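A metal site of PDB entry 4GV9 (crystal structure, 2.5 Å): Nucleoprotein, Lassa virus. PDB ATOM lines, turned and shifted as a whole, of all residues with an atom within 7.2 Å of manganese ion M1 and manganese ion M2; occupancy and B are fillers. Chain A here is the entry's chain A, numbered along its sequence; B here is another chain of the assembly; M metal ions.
SG of Cys 178 is in hydrogen-bond range of N of Asp 33.
The backbone NH (N) of Glu 35 lies within hydrogen-bond range of the backbone carbonyl oxygen (O) of Glu 43 (2.8 Å).
OP2 of C 4 of chain B lies within hydrogen-bond range of ND1 of His 172 (3.3 Å).
The backbone NH (N) of Gly 36 sits at hydrogen-bond distance from O3' of C 4 of chain B (2.4 Å).
The guanidinium group of Arg 136 lies within salt-bridge range of OP2 of C 4 of chain B.
The guanidinium group of Arg 136 lies within salt-bridge range of the side-chain carboxylate of Asp 177, 2.8 Å away.
Ile 34 touches manganese ion M1 (O to MN, 3.7 Å).
Five residues have an atom within 4 Å of manganese ion M1: Asp 33, Ile 34, Glu 35, Asp 177 and C 4 of chain B.
The nearest printed residue that does not touch manganese ion M1 is His 172 (4.1 Å).
Gln 106 touches manganese ion M2.
Asp 110 touches manganese ion M2.
Manganese ion M1 is bound by OP1 of C 4 of chain B (1.7 Å), the side-chain carboxylate (OE2) of Glu 35 (2.1 Å), the side-chain carboxylate (OD2) of Asp 177 (2.3 Å) and the side-chain carboxylate (OD2) of Asp 33 (2.5 Å).
Manganese ion M2 is bound by OD1 of Asp 33 (2.2 Å), OP1 of C 4 of chain B (2.4 Å) and O3' of G 3 of chain B (2.5 Å).
Manganese ion M2 has three donor atoms within binding distance.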
ATOM      1  N   MET A  32     -17.118  -0.785 -15.176  1.00  0.00           N
ATOM      2  CA  MET A  32     -17.305  -0.315 -13.800  1.00  0.00           C
ATOM      3  C   MET A  32     -18.726  -0.619 -13.333  1.00  0.00           C
ATOM      4  O   MET A  32     -19.697  -0.301 -14.016  1.00  0.00           O
ATOM      5  CB  MET A  32     -17.008   1.190 -13.674  1.00  0.00           C
ATOM      6  CG  MET A  32     -17.034   1.720 -12.254  1.00  0.00           C
ATOM      7  SD  MET A  32     -16.758   3.491 -12.144  1.00  0.00           S
ATOM      8  CE  MET A  32     -16.847   3.740 -10.373  1.00  0.00           C
ATOM      9  N   ASP A  33     -18.820  -1.233 -12.165  1.00  0.00           N
ATOM     10  CA  ASP A  33     -20.115  -1.489 -11.538  1.00  0.00           C
ATOM     11  C   ASP A  33     -20.038  -1.198 -10.041  1.00  0.00           C
ATOM     12  O   ASP A  33     -18.975  -1.326  -9.428  1.00  0.00           O
ATOM     13  CB  ASP A  33     -20.569  -2.923 -11.782  1.00  0.00           C
ATOM     14  CG  ASP A  33     -22.051  -3.139 -11.478  1.00  0.00           C
ATOM     15  OD1 ASP A  33     -22.893  -2.417 -12.058  1.00  0.00           O
ATOM     16  OD2 ASP A  33     -22.361  -4.014 -10.653  1.00  0.00           O
ATOM     17  N   ILE A  34     -21.171  -0.789  -9.471  1.00  0.00           N
ATOM     18  CA  ILE A  34     -21.247  -0.513  -8.040  1.00  0.00           C
ATOM     19  C   ILE A  34     -22.393  -1.263  -7.385  1.00  0.00           C
ATOM     20  O   ILE A  34     -23.395  -1.593  -8.031  1.00  0.00           O
ATOM     21  CB  ILE A  34     -21.361   1.008  -7.741  1.00  0.00           C
ATOM     22  CG1 ILE A  34     -22.637   1.600  -8.348  1.00  0.00           C
ATOM     23  CG2 ILE A  34     -20.122   1.744  -8.217  1.00  0.00           C
ATOM     24  CD1 ILE A  34     -23.143   2.841  -7.635  1.00  0.00           C
ATOM     25  N   GLU A  35     -22.229  -1.558  -6.098  1.00  0.00           N
ATOM     26  CA  GLU A  35     -23.331  -2.014  -5.263  1.00  0.00           C
ATOM     27  C   GLU A  35     -23.627  -0.942  -4.220  1.00  0.00           C
ATOM     28  O   GLU A  35     -22.716  -0.271  -3.736  1.00  0.00           O
ATOM     29  CB  GLU A  35     -23.031  -3.370  -4.612  1.00  0.00           C
ATOM     30  CG  GLU A  35     -22.791  -4.509  -5.603  1.00  0.00           C
ATOM     31  CD  GLU A  35     -23.895  -4.671  -6.634  1.00  0.00           C
ATOM     32  OE1 GLU A  35     -25.092  -4.631  -6.266  1.00  0.00           O
ATOM     33  OE2 GLU A  35     -23.560  -4.844  -7.820  1.00  0.00           O
ATOM     34  N   GLY A  36     -24.906  -0.774  -3.906  1.00  0.00           N
ATOM     35  CA  GLY A  36     -25.375   0.347  -3.100  1.00  0.00           C
ATOM     36  C   GLY A  36     -25.785   1.514  -3.983  1.00  0.00           C
ATOM     37  O   GLY A  36     -25.557   1.487  -5.198  1.00  0.00           O
ATOM     38  N   GLU A  43     -19.885  -1.093  -2.463  1.00  0.00           N
ATOM     39  CA  GLU A  43     -18.921  -1.904  -3.207  1.00  0.00           C
ATOM     40  C   GLU A  43     -18.677  -1.295  -4.576  1.00  0.00           C
ATOM     41  O   GLU A  43     -19.612  -0.982  -5.301  1.00  0.00           O
ATOM     42  CB  GLU A  43     -19.406  -3.348  -3.344  1.00  0.00           C
ATOM     43  CG  GLU A  43     -18.380  -4.292  -3.955  1.00  0.00           C
ATOM     44  CD  GLU A  43     -18.901  -5.701  -4.178  1.00  0.00           C
ATOM     45  OE1 GLU A  43     -20.096  -5.856  -4.522  1.00  0.00           O
ATOM     46  OE2 GLU A  43     -18.122  -6.657  -4.015  1.00  0.00           O
ATOM     47  N   SER A  74     -30.682  -7.177  -3.650  1.00  0.00           N
ATOM     48  CA  SER A  74     -29.541  -7.060  -4.562  1.00  0.00           C
ATOM     49  C   SER A  74     -28.237  -7.706  -4.095  1.00  0.00           C
ATOM     50  O   SER A  74     -27.953  -8.846  -4.443  1.00  0.00           O
ATOM     51  CB  SER A  74     -29.308  -5.589  -4.962  1.00  0.00           C
ATOM     52  OG  SER A  74     -28.928  -4.809  -3.834  1.00  0.00           O
ATOM     53  N   HIS A  75     -27.453  -6.978  -3.292  1.00  0.00           N
ATOM     54  CA  HIS A  75     -26.079  -7.389  -2.985  1.00  0.00           C
ATOM     55  C   HIS A  75     -25.887  -8.441  -1.887  1.00  0.00           C
ATOM     56  O   HIS A  75     -25.005  -9.287  -1.991  1.00  0.00           O
ATOM     57  CB  HIS A  75     -25.142  -6.182  -2.769  1.00  0.00           C
ATOM     58  CG  HIS A  75     -25.680  -5.144  -1.831  1.00  0.00           C
ATOM     59  ND1 HIS A  75     -25.893  -5.378  -0.492  1.00  0.00           N
ATOM     60  CD2 HIS A  75     -26.017  -3.846  -2.036  1.00  0.00           C
ATOM     61  CE1 HIS A  75     -26.348  -4.278   0.086  1.00  0.00           C
ATOM     62  NE2 HIS A  75     -26.434  -3.334  -0.835  1.00  0.00           N
ATOM     63  N   CYS A 105     -20.502   0.032 -18.925  1.00  0.00           N
ATOM     64  CA  CYS A 105     -21.300  -0.610 -17.877  1.00  0.00           C
ATOM     65  C   CYS A 105     -22.754  -0.868 -18.292  1.00  0.00           C
ATOM     66  O   CYS A 105     -23.205  -0.384 -19.334  1.00  0.00           O
ATOM     67  CB  CYS A 105     -21.283   0.216 -16.595  1.00  0.00           C
ATOM     68  SG  CYS A 105     -21.743   1.951 -16.817  1.00  0.00           S
ATOM     69  N   GLN A 106     -23.462  -1.626 -17.468  1.00  0.00           N
ATOM     70  CA  GLN A 106     -24.888  -1.875 -17.629  1.00  0.00           C
ATOM     71  C   GLN A 106     -25.684  -0.928 -16.726  1.00  0.00           C
ATOM     72  O   GLN A 106     -25.522  -0.948 -15.501  1.00  0.00           O
ATOM     73  CB  GLN A 106     -25.213  -3.338 -17.298  1.00  0.00           C
ATOM     74  CG  GLN A 106     -26.700  -3.667 -17.169  1.00  0.00           C
ATOM     75  CD  GLN A 106     -27.421  -3.731 -18.497  1.00  0.00           C
ATOM     76  OE1 GLN A 106     -28.473  -3.128 -18.670  1.00  0.00           O
ATOM     77  NE2 GLN A 106     -26.845  -4.471 -19.443  1.00  0.00           N
ATOM     78  N   GLY A 107     -26.535  -0.105 -17.336  1.00  0.00           N
ATOM     79  CA  GLY A 107     -27.291   0.919 -16.612  1.00  0.00           C
ATOM     80  C   GLY A 107     -26.364   2.019 -16.112  1.00  0.00           C
ATOM     81  O   GLY A 107     -25.845   1.945 -15.001  1.00  0.00           O
ATOM     82  N   SER A 108     -26.168   3.031 -16.959  1.00  0.00           N
ATOM     83  CA  SER A 108     -25.165   4.073 -16.700  1.00  0.00           C
ATOM     84  C   SER A 108     -25.596   5.168 -15.720  1.00  0.00           C
ATOM     85  O   SER A 108     -24.756   5.935 -15.249  1.00  0.00           O
ATOM     86  CB  SER A 108     -24.723   4.707 -18.028  1.00  0.00           C
ATOM     87  OG  SER A 108     -25.801   5.350 -18.666  1.00  0.00           O
ATOM     88  N   ASP A 110     -26.646   5.346 -12.493  1.00  0.00           N
ATOM     89  CA  ASP A 110     -26.046   5.372 -11.156  1.00  0.00           C
ATOM     90  C   ASP A 110     -24.532   5.584 -11.196  1.00  0.00           C
ATOM     91  O   ASP A 110     -23.974   6.253 -10.322  1.00  0.00           O
ATOM     92  CB  ASP A 110     -26.401   4.096 -10.367  1.00  0.00           C
ATOM     93  CG  ASP A 110     -25.842   2.821 -11.009  1.00  0.00           C
ATOM     94  OD1 ASP A 110     -25.753   2.759 -12.255  1.00  0.00           O
ATOM     95  OD2 ASP A 110     -25.505   1.891 -10.256  1.00  0.00           O
ATOM     96  N   ILE A 111     -23.892   5.040 -12.223  1.00  0.00           N
ATOM     97  CA  ILE A 111     -22.455   5.209 -12.434  1.00  0.00           C
ATOM     98  C   ILE A 111     -22.123   6.678 -12.750  1.00  0.00           C
ATOM     99  O   ILE A 111     -21.143   7.219 -12.239  1.00  0.00           O
ATOM    100  CB  ILE A 111     -21.924   4.278 -13.553  1.00  0.00           C
ATOM    101  CG1 ILE A 111     -22.250   2.803 -13.258  1.00  0.00           C
ATOM    102  CG2 ILE A 111     -20.424   4.477 -13.798  1.00  0.00           C
ATOM    103  CD1 ILE A 111     -21.588   2.213 -12.027  1.00  0.00           C
ATOM    104  N   ARG A 136     -26.818 -11.411 -17.724  1.00  0.00           N
ATOM    105  CA  ARG A 136     -26.456 -12.420 -16.734  1.00  0.00           C
ATOM    106  C   ARG A 136     -26.557 -13.853 -17.281  1.00  0.00           C
ATOM    107  O   ARG A 136     -26.965 -14.771 -16.571  1.00  0.00           O
ATOM    108  CB  ARG A 136     -27.315 -12.264 -15.471  1.00  0.00           C
ATOM    109  CG  ARG A 136     -27.226 -10.875 -14.860  1.00  0.00           C
ATOM    110  CD  ARG A 136     -27.949 -10.775 -13.529  1.00  0.00           C
ATOM    111  NE  ARG A 136     -27.839  -9.414 -12.990  1.00  0.00           N
ATOM    112  CZ  ARG A 136     -26.812  -8.968 -12.280  1.00  0.00           C
ATOM    113  NH1 ARG A 136     -25.775  -9.760 -12.004  1.00  0.00           N
ATOM    114  NH2 ARG A 136     -26.798  -7.715 -11.844  1.00  0.00           N
ATOM    115  N   HIS A 172     -25.767  -9.977  -5.967  1.00  0.00           N
ATOM    116  CA  HIS A 172     -25.112  -9.061  -6.905  1.00  0.00           C
ATOM    117  C   HIS A 172     -23.755  -8.608  -6.375  1.00  0.00           C
ATOM    118  O   HIS A 172     -23.672  -8.014  -5.293  1.00  0.00           O
ATOM    119  CB  HIS A 172     -26.006  -7.839  -7.155  1.00  0.00           C
ATOM    120  CG  HIS A 172     -27.175  -8.108  -8.047  1.00  0.00           C
ATOM    121  ND1 HIS A 172     -27.758  -7.130  -8.815  1.00  0.00           N
ATOM    122  CD2 HIS A 172     -27.864  -9.247  -8.302  1.00  0.00           C
ATOM    123  CE1 HIS A 172     -28.767  -7.647  -9.498  1.00  0.00           C
ATOM    124  NE2 HIS A 172     -28.851  -8.936  -9.213  1.00  0.00           N
ATOM    125  N   CYS A 173     -22.708  -8.888  -7.133  1.00  0.00           N
ATOM    126  CA  CYS A 173     -21.371  -8.427  -6.807  1.00  0.00           C
ATOM    127  C   CYS A 173     -20.863  -7.487  -7.889  1.00  0.00           C
ATOM    128  O   CYS A 173     -20.951  -7.797  -9.076  1.00  0.00           O
ATOM    129  CB  CYS A 173     -20.417  -9.620  -6.669  1.00  0.00           C
ATOM    130  SG  CYS A 173     -18.724  -9.165  -6.220  1.00  0.00           S
ATOM    131  N   ALA A 174     -20.339  -6.340  -7.481  1.00  0.00           N
ATOM    132  CA  ALA A 174     -19.821  -5.335  -8.405  1.00  0.00           C
ATOM    133  C   ALA A 174     -18.717  -5.890  -9.308  1.00  0.00           C
ATOM    134  O   ALA A 174     -18.655  -5.537 -10.492  1.00  0.00           O
ATOM    135  CB  ALA A 174     -19.318  -4.115  -7.631  1.00  0.00           C
ATOM    136  N   LEU A 175     -17.876  -6.750  -8.753  1.00  0.00           N
ATOM    137  CA  LEU A 175     -16.778  -7.370  -9.506  1.00  0.00           C
ATOM    138  C   LEU A 175     -17.279  -8.454 -10.463  1.00  0.00           C
ATOM    139  O   LEU A 175     -16.883  -8.474 -11.630  1.00  0.00           O
ATOM    140  CB  LEU A 175     -15.706  -7.920  -8.559  1.00  0.00           C
ATOM    141  CG  LEU A 175     -14.460  -8.588  -9.150  1.00  0.00           C
ATOM    142  CD1 LEU A 175     -13.703  -7.655 -10.087  1.00  0.00           C
ATOM    143  CD2 LEU A 175     -13.543  -9.090  -8.050  1.00  0.00           C
ATOM    144  N   ASP A 177     -20.298  -8.803 -11.627  1.00  0.00           N
ATOM    145  CA  ASP A 177     -21.109  -8.130 -12.642  1.00  0.00           C
ATOM    146  C   ASP A 177     -20.250  -7.646 -13.802  1.00  0.00           C
ATOM    147  O   ASP A 177     -20.573  -7.897 -14.966  1.00  0.00           O
ATOM    148  CB  ASP A 177     -21.903  -6.980 -12.031  1.00  0.00           C
ATOM    149  CG  ASP A 177     -23.156  -7.444 -11.292  1.00  0.00           C
ATOM    150  OD1 ASP A 177     -23.360  -8.673 -11.145  1.00  0.00           O
ATOM    151  OD2 ASP A 177     -23.947  -6.573 -10.861  1.00  0.00           O
ATOM    152  N   CYS A 178     -19.143  -6.963 -13.488  1.00  0.00           N
ATOM    153  CA  CYS A 178     -18.200  -6.476 -14.493  1.00  0.00           C
ATOM    154  C   CYS A 178     -17.697  -7.594 -15.415  1.00  0.00           C
ATOM    155  O   CYS A 178     -17.589  -7.409 -16.620  1.00  0.00           O
ATOM    156  CB  CYS A 178     -17.012  -5.773 -13.824  1.00  0.00           C
ATOM    157  SG  CYS A 178     -17.348  -4.093 -13.270  1.00  0.00           S
ATOM    158  N   PHE A 181     -20.863  -9.126 -17.462  1.00  0.00           N
ATOM    159  CA  PHE A 181     -21.337  -8.185 -18.488  1.00  0.00           C
ATOM    160  C   PHE A 181     -20.402  -8.209 -19.697  1.00  0.00           C
ATOM    161  O   PHE A 181     -20.858  -8.104 -20.841  1.00  0.00           O
ATOM    162  CB  PHE A 181     -21.440  -6.753 -17.949  1.00  0.00           C
ATOM    163  CG  PHE A 181     -22.453  -6.570 -16.843  1.00  0.00           C
ATOM    164  CD1 PHE A 181     -23.574  -7.391 -16.738  1.00  0.00           C
ATOM    165  CD2 PHE A 181     -22.296  -5.532 -15.926  1.00  0.00           C
ATOM    166  CE1 PHE A 181     -24.500  -7.200 -15.716  1.00  0.00           C
ATOM    167  CE2 PHE A 181     -23.216  -5.330 -14.910  1.00  0.00           C
ATOM    168  CZ  PHE A 181     -24.320  -6.165 -14.801  1.00  0.00           C
ATOM    169  P     G B   3     -30.063  -4.251 -14.614  1.00  0.00           P
ATOM    170  OP1   G B   3     -28.728  -4.748 -15.018  1.00  0.00           O
ATOM    171  OP2   G B   3     -31.048  -5.192 -14.036  1.00  0.00           O
ATOM    172  O5'   G B   3     -29.871  -3.045 -13.598  1.00  0.00           O
ATOM    173  C5'   G B   3     -28.911  -2.003 -13.840  1.00  0.00           C
ATOM    174  C4'   G B   3     -28.898  -1.007 -12.705  1.00  0.00           C
ATOM    175  O4'   G B   3     -30.179  -0.326 -12.630  1.00  0.00           O
ATOM    176  C3'   G B   3     -28.711  -1.590 -11.307  1.00  0.00           C
ATOM    177  O3'   G B   3     -27.355  -1.884 -10.997  1.00  0.00           O
ATOM    178  C2'   G B   3     -29.309  -0.497 -10.438  1.00  0.00           C
ATOM    179  O2'   G B   3     -28.439   0.606 -10.224  1.00  0.00           O
ATOM    180  C1'   G B   3     -30.514  -0.068 -11.276  1.00  0.00           C
ATOM    181  N9    G B   3     -31.718  -0.838 -10.944  1.00  0.00           N
ATOM    182  C8    G B   3     -32.258  -1.880 -11.658  1.00  0.00           C
ATOM    183  N7    G B   3     -33.326  -2.376 -11.112  1.00  0.00           N
ATOM    184  C5    G B   3     -33.512  -1.613  -9.968  1.00  0.00           C
ATOM    185  C6    G B   3     -34.525  -1.687  -8.963  1.00  0.00           C
ATOM    186  O6    G B   3     -35.480  -2.461  -8.891  1.00  0.00           O
ATOM    187  N1    G B   3     -34.333  -0.722  -7.978  1.00  0.00           N
ATOM    188  C2    G B   3     -33.306   0.186  -7.954  1.00  0.00           C
ATOM    189  N2    G B   3     -33.289   1.039  -6.919  1.00  0.00           N
ATOM    190  N3    G B   3     -32.357   0.259  -8.876  1.00  0.00           N
ATOM    191  C4    G B   3     -32.521  -0.661  -9.851  1.00  0.00           C
ATOM    192  P     C B   4     -27.007  -3.186 -10.120  1.00  0.00           P
ATOM    193  OP1   C B   4     -25.533  -3.406 -10.198  1.00  0.00           O
ATOM    194  OP2   C B   4     -27.931  -4.282 -10.508  1.00  0.00           O
ATOM    195  O5'   C B   4     -27.378  -2.726  -8.635  1.00  0.00           O
ATOM    196  C5'   C B   4     -26.725  -1.593  -8.023  1.00  0.00           C
ATOM    197  C4'   C B   4     -27.461  -1.170  -6.782  1.00  0.00           C
ATOM    198  O4'   C B   4     -28.825  -0.806  -7.116  1.00  0.00           O
ATOM    199  C3'   C B   4     -27.625  -2.230  -5.701  1.00  0.00           C
ATOM    200  O3'   C B   4     -26.462  -2.348  -4.880  1.00  0.00           O
ATOM    201  C2'   C B   4     -28.813  -1.709  -4.914  1.00  0.00           C
ATOM    202  O2'   C B   4     -28.494  -0.698  -3.979  1.00  0.00           O
ATOM    203  C1'   C B   4     -29.694  -1.144  -6.043  1.00  0.00           C
ATOM    204  N1    C B   4     -30.694  -2.113  -6.528  1.00  0.00           N
ATOM    205  C2    C B   4     -31.887  -2.267  -5.820  1.00  0.00           C
ATOM    206  O2    C B   4     -32.076  -1.578  -4.800  1.00  0.00           O
ATOM    207  N3    C B   4     -32.810  -3.154  -6.258  1.00  0.00           N
ATOM    208  C4    C B   4     -32.568  -3.875  -7.350  1.00  0.00           C
ATOM    209  N4    C B   4     -33.503  -4.749  -7.747  1.00  0.00           N
ATOM    210  C5    C B   4     -31.355  -3.745  -8.098  1.00  0.00           C
ATOM    211  C6    C B   4     -30.458  -2.857  -7.648  1.00  0.00           C
HETATM  212 MN    MN M   1     -24.546  -4.711  -9.693  1.00  0.00          MN
HETATM  213 MN    MN M   2     -24.931  -1.655 -11.744  1.00  0.00          MN
